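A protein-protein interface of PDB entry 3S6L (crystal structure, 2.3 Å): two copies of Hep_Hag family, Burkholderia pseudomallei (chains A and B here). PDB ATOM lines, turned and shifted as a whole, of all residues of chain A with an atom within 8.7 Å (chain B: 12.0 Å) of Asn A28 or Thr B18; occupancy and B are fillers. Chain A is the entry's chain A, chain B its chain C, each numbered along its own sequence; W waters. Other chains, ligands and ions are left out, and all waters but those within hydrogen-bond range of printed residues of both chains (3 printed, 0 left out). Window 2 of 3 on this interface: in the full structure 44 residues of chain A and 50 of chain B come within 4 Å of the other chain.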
ATOM      1  N   ARG A  17      15.808  16.248  -6.178  1.00  0.00           N
ATOM      2  CA  ARG A  17      15.006  16.066  -4.969  1.00  0.00           C
ATOM      3  C   ARG A  17      13.536  16.373  -5.267  1.00  0.00           C
ATOM      4  O   ARG A  17      13.222  17.283  -6.043  1.00  0.00           O
ATOM      5  CB  ARG A  17      15.543  16.918  -3.806  1.00  0.00           C
ATOM      6  CG  ARG A  17      17.065  16.791  -3.611  1.00  0.00           C
ATOM      7  CD  ARG A  17      17.673  17.833  -2.656  1.00  0.00           C
ATOM      8  NE  ARG A  17      17.855  19.173  -3.249  1.00  0.00           N
ATOM      9  CZ  ARG A  17      18.782  19.510  -4.158  1.00  0.00           C
ATOM     10  NH1 ARG A  17      19.652  18.621  -4.649  1.00  0.00           N
ATOM     11  NH2 ARG A  17      18.845  20.765  -4.565  1.00  0.00           N
ATOM     12  N   SER A  25      13.622  19.915  -7.399  1.00  0.00           N
ATOM     13  CA  SER A  25      14.845  20.712  -7.487  1.00  0.00           C
ATOM     14  C   SER A  25      16.064  19.886  -7.873  1.00  0.00           C
ATOM     15  O   SER A  25      16.195  18.722  -7.479  1.00  0.00           O
ATOM     16  CB  SER A  25      15.119  21.440  -6.184  1.00  0.00           C
ATOM     17  OG  SER A  25      15.245  20.506  -5.180  1.00  0.00           O
ATOM     18  N   ALA A  26      16.953  20.506  -8.652  1.00  0.00           N
ATOM     19  CA  ALA A  26      18.236  19.903  -9.021  1.00  0.00           C
ATOM     20  C   ALA A  26      19.291  21.000  -9.104  1.00  0.00           C
ATOM     21  O   ALA A  26      19.027  22.079  -9.679  1.00  0.00           O
ATOM     22  CB  ALA A  26      18.121  19.171 -10.348  1.00  0.00           C
ATOM     23  N   GLY A  27      20.472  20.709  -8.557  1.00  0.00           N
ATOM     24  CA  GLY A  27      21.607  21.646  -8.548  1.00  0.00           C
ATOM     25  C   GLY A  27      22.083  21.856  -7.126  1.00  0.00           C
ATOM     26  O   GLY A  27      21.311  21.655  -6.193  1.00  0.00           O
ATOM     27  N   ASN A  28      23.354  22.221  -6.940  1.00  0.00           N
ATOM     28  CA  ASN A  28      23.843  22.539  -5.596  1.00  0.00           C
ATOM     29  C   ASN A  28      23.036  23.660  -4.960  1.00  0.00           C
ATOM     30  O   ASN A  28      22.991  24.772  -5.504  1.00  0.00           O
ATOM     31  CB  ASN A  28      25.334  22.885  -5.605  1.00  0.00           C
ATOM     32  CG  ASN A  28      26.213  21.644  -5.653  1.00  0.00           C
ATOM     33  OD1 ASN A  28      25.773  20.513  -5.295  1.00  0.00           O
ATOM     34  ND2 ASN A  28      27.467  21.830  -6.088  1.00  0.00           N
ATOM     35  N   GLY A  29      22.371  23.353  -3.834  1.00  0.00           N
ATOM     36  CA  GLY A  29      21.600  24.366  -3.091  1.00  0.00           C
ATOM     37  C   GLY A  29      20.302  24.784  -3.788  1.00  0.00           C
ATOM     38  O   GLY A  29      19.704  25.792  -3.431  1.00  0.00           O
ATOM     39  N   ALA A  30      19.859  24.020  -4.783  1.00  0.00           N
ATOM     40  CA  ALA A  30      18.574  24.294  -5.430  1.00  0.00           C
ATOM     41  C   ALA A  30      17.415  23.990  -4.480  1.00  0.00           C
ATOM     42  O   ALA A  30      17.456  23.025  -3.732  1.00  0.00           O
ATOM     43  CB  ALA A  30      18.447  23.483  -6.706  1.00  0.00           C
ATOM     44  N   ASN A  31      16.387  24.826  -4.482  1.00  0.00           N
ATOM     45  CA  ASN A  31      15.300  24.639  -3.522  1.00  0.00           C
ATOM     46  C   ASN A  31      13.960  25.145  -4.033  1.00  0.00           C
ATOM     47  O   ASN A  31      13.802  26.311  -4.418  1.00  0.00           O
ATOM     48  CB  ASN A  31      15.636  25.225  -2.138  1.00  0.00           C
ATOM     49  CG  ASN A  31      14.670  24.738  -1.031  1.00  0.00           C
ATOM     50  OD1 ASN A  31      14.116  23.622  -1.095  1.00  0.00           O
ATOM     51  ND2 ASN A  31      14.483  25.573   0.007  1.00  0.00           N
ATOM     52  N   ALA A  39      12.840  24.165  -9.401  1.00  0.00           N
ATOM     53  CA  ALA A  39      13.995  25.034  -9.226  1.00  0.00           C
ATOM     54  C   ALA A  39      15.177  24.262  -9.741  1.00  0.00           C
ATOM     55  O   ALA A  39      15.574  23.251  -9.135  1.00  0.00           O
ATOM     56  CB  ALA A  39      14.194  25.435  -7.720  1.00  0.00           C
ATOM     57  N   VAL A  40      15.742  24.725 -10.845  1.00  0.00           N
ATOM     58  CA  VAL A  40      16.832  23.996 -11.470  1.00  0.00           C
ATOM     59  C   VAL A  40      18.028  24.901 -11.731  1.00  0.00           C
ATOM     60  O   VAL A  40      17.906  25.912 -12.412  1.00  0.00           O
ATOM     61  CB  VAL A  40      16.336  23.228 -12.739  1.00  0.00           C
ATOM     62  CG1 VAL A  40      17.522  22.517 -13.458  1.00  0.00           C
ATOM     63  CG2 VAL A  40      15.280  22.188 -12.331  1.00  0.00           C
ATOM     64  N   GLY A  41      19.172  24.528 -11.154  1.00  0.00           N
ATOM     65  CA  GLY A  41      20.386  25.321 -11.229  1.00  0.00           C
ATOM     66  C   GLY A  41      21.065  25.586  -9.878  1.00  0.00           C
ATOM     67  O   GLY A  41      20.449  25.470  -8.809  1.00  0.00           O
ATOM     68  N   GLY A  42      22.338  25.961  -9.942  1.00  0.00           N
ATOM     69  CA  GLY A  42      23.112  26.280  -8.727  1.00  0.00           C
ATOM     70  C   GLY A  42      22.438  27.394  -7.950  1.00  0.00           C
ATOM     71  O   GLY A  42      22.219  28.493  -8.481  1.00  0.00           O
ATOM     72  N   ALA A  43      22.094  27.098  -6.699  1.00  0.00           N
ATOM     73  CA  ALA A  43      21.397  28.051  -5.848  1.00  0.00           C
ATOM     74  C   ALA A  43      20.093  28.583  -6.472  1.00  0.00           C
ATOM     75  O   ALA A  43      19.602  29.626  -6.047  1.00  0.00           O
ATOM     76  CB  ALA A  43      22.353  29.230  -5.415  1.00  0.00           C
ATOM     77  N   ALA A  44      19.516  27.864  -7.450  1.00  0.00           N
ATOM     78  CA  ALA A  44      18.185  28.230  -7.948  1.00  0.00           C
ATOM     79  C   ALA A  44      17.151  28.149  -6.830  1.00  0.00           C
ATOM     80  O   ALA A  44      17.159  27.212  -6.020  1.00  0.00           O
ATOM     81  CB  ALA A  44      17.766  27.342  -9.107  1.00  0.00           C
ATOM     82  N   SER A  45      16.218  29.095  -6.813  1.00  0.00           N
ATOM     83  CA  SER A  45      15.228  29.098  -5.753  1.00  0.00           C
ATOM     84  C   SER A  45      13.788  29.315  -6.251  1.00  0.00           C
ATOM     85  O   SER A  45      13.510  30.218  -7.017  1.00  0.00           O
ATOM     86  CB  SER A  45      15.650  30.114  -4.686  1.00  0.00           C
ATOM     87  OG  SER A  45      14.626  30.263  -3.745  1.00  0.00           O
ATOM     88  N   GLY A  55      18.059  28.222 -13.807  1.00  0.00           N
ATOM     89  CA  GLY A  55      19.332  28.924 -13.960  1.00  0.00           C
ATOM     90  C   GLY A  55      20.022  29.194 -12.637  1.00  0.00           C
ATOM     91  O   GLY A  55      19.369  29.210 -11.590  1.00  0.00           O
ATOM     92  N   GLN A  56      21.337  29.403 -12.669  1.00  0.00           N
ATOM     93  CA  GLN A  56      22.096  29.630 -11.424  1.00  0.00           C
ATOM     94  C   GLN A  56      21.639  30.961 -10.780  1.00  0.00           C
ATOM     95  O   GLN A  56      21.422  31.958 -11.455  1.00  0.00           O
ATOM     96  CB  GLN A  56      23.620  29.611 -11.686  1.00  0.00           C
ATOM     97  CG  GLN A  56      24.519  29.491 -10.438  1.00  0.00           C
ATOM     98  CD  GLN A  56      24.710  30.807  -9.689  1.00  0.00           C
ATOM     99  OE1 GLN A  56      24.671  31.899 -10.273  1.00  0.00           O
ATOM    100  NE2 GLN A  56      24.909  30.705  -8.381  1.00  0.00           N
ATOM    101  N   ALA A  57      21.487  30.955  -9.472  1.00  0.00           N
ATOM    102  CA  ALA A  57      20.921  32.093  -8.714  1.00  0.00           C
ATOM    103  C   ALA A  57      19.542  32.616  -9.192  1.00  0.00           C
ATOM    104  O   ALA A  57      19.122  33.702  -8.779  1.00  0.00           O
ATOM    105  CB  ALA A  57      21.962  33.260  -8.533  1.00  0.00           C
ATOM    106  N   VAL B  16      22.595  14.252 -12.650  1.00  0.00           N
ATOM    107  CA  VAL B  16      22.839  15.723 -12.383  1.00  0.00           C
ATOM    108  C   VAL B  16      24.292  16.038 -12.063  1.00  0.00           C
ATOM    109  O   VAL B  16      24.745  15.768 -10.967  1.00  0.00           O
ATOM    110  CB  VAL B  16      21.928  16.327 -11.259  1.00  0.00           C
ATOM    111  CG1 VAL B  16      22.113  17.856 -11.151  1.00  0.00           C
ATOM    112  CG2 VAL B  16      20.447  16.057 -11.509  1.00  0.00           C
ATOM    113  N   ARG B  17      25.023  16.622 -13.006  1.00  0.00           N
ATOM    114  CA  ARG B  17      26.426  16.959 -12.777  1.00  0.00           C
ATOM    115  C   ARG B  17      26.563  18.449 -12.387  1.00  0.00           C
ATOM    116  O   ARG B  17      25.874  19.329 -12.954  1.00  0.00           O
ATOM    117  CB  ARG B  17      27.288  16.633 -14.009  1.00  0.00           C
ATOM    118  CG  ARG B  17      27.228  15.138 -14.464  1.00  0.00           C
ATOM    119  CD  ARG B  17      27.773  14.907 -15.896  1.00  0.00           C
ATOM    120  NE  ARG B  17      26.984  15.509 -16.991  1.00  0.00           N
ATOM    121  CZ  ARG B  17      25.768  15.111 -17.395  1.00  0.00           C
ATOM    122  NH1 ARG B  17      25.140  14.102 -16.808  1.00  0.00           N
ATOM    123  NH2 ARG B  17      25.170  15.730 -18.410  1.00  0.00           N
ATOM    124  N   THR B  18      27.434  18.716 -11.411  1.00  0.00           N
ATOM    125  CA  THR B  18      27.663  20.073 -10.905  1.00  0.00           C
ATOM    126  C   THR B  18      29.145  20.364 -10.780  1.00  0.00           C
ATOM    127  O   THR B  18      29.941  19.464 -10.498  1.00  0.00           O
ATOM    128  CB  THR B  18      27.043  20.289  -9.515  1.00  0.00           C
ATOM    129  OG1 THR B  18      27.707  19.437  -8.570  1.00  0.00           O
ATOM    130  CG2 THR B  18      25.527  20.020  -9.526  1.00  0.00           C
ATOM    131  N   SER B  19      29.518  21.618 -10.998  1.00  0.00           N
ATOM    132  CA  SER B  19      30.916  22.038 -10.866  1.00  0.00           C
ATOM    133  C   SER B  19      31.017  23.036  -9.714  1.00  0.00           C
ATOM    134  O   SER B  19      29.993  23.586  -9.246  1.00  0.00           O
ATOM    135  CB  SER B  19      31.407  22.702 -12.160  1.00  0.00           C
ATOM    136  OG  SER B  19      30.867  24.016 -12.295  1.00  0.00           O
ATOM    137  N   SER B  20      32.252  23.304  -9.292  1.00  0.00           N
ATOM    138  CA  SER B  20      32.505  24.245  -8.202  1.00  0.00           C
ATOM    139  C   SER B  20      32.290  25.682  -8.666  1.00  0.00           C
ATOM    140  O   SER B  20      32.217  26.586  -7.833  1.00  0.00           O
ATOM    141  CB  SER B  20      33.925  24.069  -7.605  1.00  0.00           C
ATOM    142  OG  SER B  20      34.915  23.887  -8.627  1.00  0.00           O
ATOM    143  N   LEU B  21      32.157  25.884  -9.983  1.00  0.00           N
ATOM    144  CA  LEU B  21      31.983  27.222 -10.558  1.00  0.00           C
ATOM    145  C   LEU B  21      30.526  27.575 -10.946  1.00  0.00           C
ATOM    146  O   LEU B  21      30.298  28.464 -11.780  1.00  0.00           O
ATOM    147  CB  LEU B  21      32.966  27.430 -11.726  1.00  0.00           C
ATOM    148  CG  LEU B  21      34.486  27.433 -11.412  1.00  0.00           C
ATOM    149  CD1 LEU B  21      35.369  27.513 -12.691  1.00  0.00           C
ATOM    150  CD2 LEU B  21      34.916  28.555 -10.430  1.00  0.00           C
ATOM    151  N   GLY B  22      29.562  26.878 -10.332  1.00  0.00           N
ATOM    152  CA  GLY B  22      28.128  27.142 -10.479  1.00  0.00           C
ATOM    153  C   GLY B  22      27.405  26.473 -11.653  1.00  0.00           C
ATOM    154  O   GLY B  22      26.271  26.835 -11.960  1.00  0.00           O
ATOM    155  N   ASP B  23      28.057  25.506 -12.301  1.00  0.00           N
ATOM    156  CA  ASP B  23      27.512  24.842 -13.471  1.00  0.00           C
ATOM    157  C   ASP B  23      26.656  23.665 -13.045  1.00  0.00           C
ATOM    158  O   ASP B  23      27.029  22.942 -12.094  1.00  0.00           O
ATOM    159  CB  ASP B  23      28.612  24.373 -14.429  1.00  0.00           C
ATOM    160  CG  ASP B  23      29.509  25.526 -14.924  1.00  0.00           C
ATOM    161  OD1 ASP B  23      29.015  26.491 -15.583  1.00  0.00           O
ATOM    162  OD2 ASP B  23      30.728  25.471 -14.644  1.00  0.00           O
ATOM    163  N   THR B  24      25.522  23.480 -13.742  1.00  0.00           N
ATOM    164  CA  THR B  24      24.624  22.343 -13.519  1.00  0.00           C
ATOM    165  C   THR B  24      24.266  21.710 -14.874  1.00  0.00           C
ATOM    166  O   THR B  24      23.858  22.426 -15.806  1.00  0.00           O
ATOM    167  CB  THR B  24      23.290  22.777 -12.810  1.00  0.00           C
ATOM    168  OG1 THR B  24      23.556  23.600 -11.651  1.00  0.00           O
ATOM    169  CG2 THR B  24      22.437  21.558 -12.410  1.00  0.00           C
ATOM    170  N   SER B  25      24.407  20.384 -14.981  1.00  0.00           N
ATOM    171  CA  SER B  25      24.127  19.646 -16.229  1.00  0.00           C
ATOM    172  C   SER B  25      23.257  18.413 -16.009  1.00  0.00           C
ATOM    173  O   SER B  25      23.489  17.635 -15.082  1.00  0.00           O
ATOM    174  CB  SER B  25      25.431  19.193 -16.879  1.00  0.00           C
ATOM    175  OG  SER B  25      26.109  20.297 -17.448  1.00  0.00           O
ATOM    176  N   ALA B  26      22.269  18.223 -16.875  1.00  0.00           N
ATOM    177  CA  ALA B  26      21.393  17.039 -16.829  1.00  0.00           C
ATOM    178  C   ALA B  26      20.946  16.674 -18.230  1.00  0.00           C
ATOM    179  O   ALA B  26      20.471  17.517 -18.990  1.00  0.00           O
ATOM    180  CB  ALA B  26      20.186  17.283 -15.926  1.00  0.00           C
ATOM    181  N   GLY B  27      21.115  15.408 -18.578  1.00  0.00           N
ATOM    182  CA  GLY B  27      20.795  14.952 -19.914  1.00  0.00           C
ATOM    183  C   GLY B  27      21.995  14.291 -20.546  1.00  0.00           C
ATOM    184  O   GLY B  27      23.133  14.562 -20.182  1.00  0.00           O
ATOM    185  N   GLY B  29      24.940  13.920 -22.582  1.00  0.00           N
ATOM    186  CA  GLY B  29      25.845  14.881 -23.254  1.00  0.00           C
ATOM    187  C   GLY B  29      25.630  16.368 -22.927  1.00  0.00           C
ATOM    188  O   GLY B  29      26.315  17.235 -23.484  1.00  0.00           O
ATOM    189  N   ALA B  30      24.690  16.662 -22.023  1.00  0.00           N
ATOM    190  CA  ALA B  30      24.437  18.035 -21.574  1.00  0.00           C
ATOM    191  C   ALA B  30      25.679  18.625 -20.920  1.00  0.00           C
ATOM    192  O   ALA B  30      26.322  17.985 -20.086  1.00  0.00           O
ATOM    193  CB  ALA B  30      23.274  18.073 -20.615  1.00  0.00           C
ATOM    194  N   ASN B  31      26.036  19.845 -21.297  1.00  0.00           N
ATOM    195  CA  ASN B  31      27.302  20.414 -20.823  1.00  0.00           C
ATOM    196  C   ASN B  31      27.190  21.904 -20.567  1.00  0.00           C
ATOM    197  O   ASN B  31      27.027  22.701 -21.492  1.00  0.00           O
ATOM    198  CB  ASN B  31      28.461  20.098 -21.789  1.00  0.00           C
ATOM    199  CG  ASN B  31      29.852  20.495 -21.220  1.00  0.00           C
ATOM    200  OD1 ASN B  31      30.015  20.763 -20.021  1.00  0.00           O
ATOM    201  ND2 ASN B  31      30.856  20.506 -22.092  1.00  0.00           N
ATOM    202  N   ALA B  32      27.232  22.256 -19.289  1.00  0.00           N
ATOM    203  CA  ALA B  32      27.370  23.643 -18.859  1.00  0.00           C
ATOM    204  C   ALA B  32      28.818  23.866 -18.425  1.00  0.00           C
ATOM    205  O   ALA B  32      29.258  23.310 -17.430  1.00  0.00           O
ATOM    206  CB  ALA B  32      26.424  23.924 -17.728  1.00  0.00           C
ATOM    207  N   SER B  33      29.560  24.668 -19.176  1.00  0.00           N
ATOM    208  CA  SER B  33      30.999  24.784 -18.957  1.00  0.00           C
ATOM    209  C   SER B  33      31.473  26.221 -18.817  1.00  0.00           C
ATOM    210  O   SER B  33      32.697  26.468 -18.700  1.00  0.00           O
ATOM    211  CB  SER B  33      31.734  24.157 -20.131  1.00  0.00           C
ATOM    212  OG  SER B  33      31.344  24.815 -21.329  1.00  0.00           O
ATOM    213  N   GLY B  34      30.548  27.183 -18.826  1.00  0.00           N
ATOM    214  CA  GLY B  34      30.961  28.575 -18.871  1.00  0.00           C
ATOM    215  C   GLY B  34      31.068  29.330 -17.545  1.00  0.00           C
ATOM    216  O   GLY B  34      31.512  30.485 -17.539  1.00  0.00           O
ATOM    217  N   GLY B  35      30.671  28.710 -16.430  1.00  0.00           N
ATOM    218  CA  GLY B  35      30.616  29.429 -15.140  1.00  0.00           C
ATOM    219  C   GLY B  35      29.178  29.869 -14.937  1.00  0.00           C
ATOM    220  O   GLY B  35      28.612  30.540 -15.805  1.00  0.00           O
ATOM    221  N   ASN B  36      28.588  29.484 -13.800  1.00  0.00           N
ATOM    222  CA  ASN B  36      27.164  29.701 -13.523  1.00  0.00           C
ATOM    223  C   ASN B  36      26.265  29.254 -14.690  1.00  0.00           C
ATOM    224  O   ASN B  36      25.257  29.880 -14.985  1.00  0.00           O
ATOM    225  CB  ASN B  36      26.870  31.156 -13.138  1.00  0.00           C
ATOM    226  CG  ASN B  36      27.569  31.579 -11.856  1.00  0.00           C
ATOM    227  OD1 ASN B  36      27.745  30.777 -10.936  1.00  0.00           O
ATOM    228  ND2 ASN B  36      27.977  32.859 -11.792  1.00  0.00           N
ATOM    229  N   GLY B  37      26.649  28.168 -15.356  1.00  0.00           N
ATOM    230  CA  GLY B  37      25.865  27.668 -16.489  1.00  0.00           C
ATOM    231  C   GLY B  37      24.839  26.652 -16.044  1.00  0.00           C
ATOM    232  O   GLY B  37      25.026  25.964 -15.053  1.00  0.00           O
ATOM    233  N   THR B  38      23.738  26.557 -16.772  1.00  0.00           N
ATOM    234  CA  THR B  38      22.777  25.497 -16.539  1.00  0.00           C
ATOM    235  C   THR B  38      22.424  24.917 -17.912  1.00  0.00           C
ATOM    236  O   THR B  38      22.038  25.670 -18.814  1.00  0.00           O
ATOM    237  CB  THR B  38      21.553  26.033 -15.791  1.00  0.00           C
ATOM    238  OG1 THR B  38      21.968  26.653 -14.557  1.00  0.00           O
ATOM    239  CG2 THR B  38      20.541  24.933 -15.509  1.00  0.00           C
ATOM    240  N   ALA B  39      22.597  23.604 -18.083  1.00  0.00           N
ATOM    241  CA  ALA B  39      22.283  22.947 -19.365  1.00  0.00           C
ATOM    242  C   ALA B  39      21.465  21.700 -19.120  1.00  0.00           C
ATOM    243  O   ALA B  39      21.940  20.785 -18.451  1.00  0.00           O
ATOM    244  CB  ALA B  39      23.550  22.597 -20.120  1.00  0.00           C
ATOM    245  N   VAL B  40      20.247  21.653 -19.654  1.00  0.00           N
ATOM    246  CA  VAL B  40      19.324  20.554 -19.361  1.00  0.00           C
ATOM    247  C   VAL B  40      18.603  20.104 -20.643  1.00  0.00           C
ATOM    248  O   VAL B  40      17.850  20.889 -21.246  1.00  0.00           O
ATOM    249  CB  VAL B  40      18.258  20.961 -18.279  1.00  0.00           C
ATOM    250  CG1 VAL B  40      17.237  19.823 -18.047  1.00  0.00           C
ATOM    251  CG2 VAL B  40      18.931  21.348 -16.937  1.00  0.00           C
ATOM    252  N   ALA B  46      25.642  24.932 -22.604  1.00  0.00           N
ATOM    253  CA  ALA B  46      25.705  26.292 -22.063  1.00  0.00           C
ATOM    254  C   ALA B  46      27.192  26.620 -21.913  1.00  0.00           C
ATOM    255  O   ALA B  46      27.820  26.297 -20.877  1.00  0.00           O
ATOM    256  CB  ALA B  46      24.974  26.379 -20.725  1.00  0.00           C
HETATM  257  O   HOH W   1      23.784  26.196 -12.355  1.00  0.00           O
HETATM  258  O   HOH W   2      24.672  23.171  -9.226  1.00  0.00           O
HETATM  259  O   HOH W   3      22.523  29.208 -15.377  1.00  0.00           O
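The side-chain hydroxyl (OG1) of Thr B18 lies within hydrogen-bond range of the side-chain amide nitrogen (ND2) of Asn A28 (3.5 Å).
The backbone NH of Gln A56 lies within hydrogen-bond range of the side-chain hydroxyl of Thr B38, at 3.4 Å.
OE1 of Gln A56 lies close to OD1 of Asn B36 (3.3 Å).
The side-chain hydroxyl (OG1) of Thr B24 lies within hydrogen-bond range of the backbone NH (N) of Gly A42 (3.2 Å).
The backbone carbonyl oxygen (O) of Gly B37 lies within hydrogen-bond range of the backbone NH (N) of Thr B24.
The backbone NH of Ala A57 sits at hydrogen-bond distance from the backbone carbonyl oxygen of Gly A42 (2.8 Å).
The backbone NH (N) of Ala B39 lies within hydrogen-bond range of the backbone carbonyl oxygen (O) of Thr B24, at 2.9 Å.
NH2 of Arg A17 lies within hydrogen-bond range of O of Gly A27 (3.1 Å).
O of Val A40 is in hydrogen-bond range of N of Gly A55, at 2.7 Å.
The backbone carbonyl oxygen (O) of Gly A42 sits close to the side-chain amide nitrogen (NE2) of Gln A56, 3.5 Å away.
Among the printed residues, merely in contact across the chains: Gly A27 with Thr B24, Val A40 with Val B40, Gly A41 with Thr B24, Gly A41 with Thr B38, Gly A55 with Thr B38 and Gln A56 with Gly B22.
Of chain B, only Thr B24 (3.95 Å) comes within 4 Å of Gly A27.
Printed residues of chain B within 4 Å of Asn A28: Thr B18 (3.5 Å).
Ala A30 touches none of the printed residues of chain B.
Of chain B, only Thr B24 (3.6 Å) and Thr B38 (3.9 Å) come within 4 Å of Gly A41.
Gly A42 touches just one residue of chain B: Thr B24.
No residue of chain B comes within 4 Å of Ala A44.
Of the printed residues of chain A, Thr B18 touches Asn A28.
No residue of chain A comes within 4 Å of Ser B19.
Of the printed residues of chain A, Thr B24 touches Gly A27, Gly A41 and Gly A42.
Of the printed residues of chain A, Asn B36 touches Gln A56 (3.3 Å).
Of the 25 printed residues of chain B, 6 touch a printed residue of chain A.
Along chain B the printed residues that touch a printed residue of chain A span positions 18 to 40.
Of the 18 printed residues of chain A, 7 touch a printed residue of chain B.
Hydrophobic or aromatic side chains of chain A within 4 Å of the printed part of chain B: Val A40.
Among the printed residues, no Asp or Glu carboxylate lies within 4 Å of a Lys or Arg side-chain nitrogen of the other chain.
Val A40 touches its own counterpart, Val B40.
Water W1 lies within hydrogen-bond range of the backbone carbonyl oxygen of Gly B22 (2.6 Å), the side-chain hydroxyl of Thr B24 (2.7 Å), the backbone NH of Gly A42 (2.8 Å), the side-chain hydroxyl of Thr B38 (2.9 Å) and the backbone carbonyl oxygen of Gly B37 (3.0 Å).
Water W2 bridges the side-chain hydroxyl of Thr B24 (2.7 Å) and the backbone NH of Asn A28 (2.8 Å).
Water W3 lies within hydrogen-bond range of the side-chain hydroxyl (OG1) of Thr B38 (2.7 Å), the backbone carbonyl oxygen (O) of Asn B36 (2.8 Å) and the backbone NH (N) of Gln A56 (3.0 Å).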
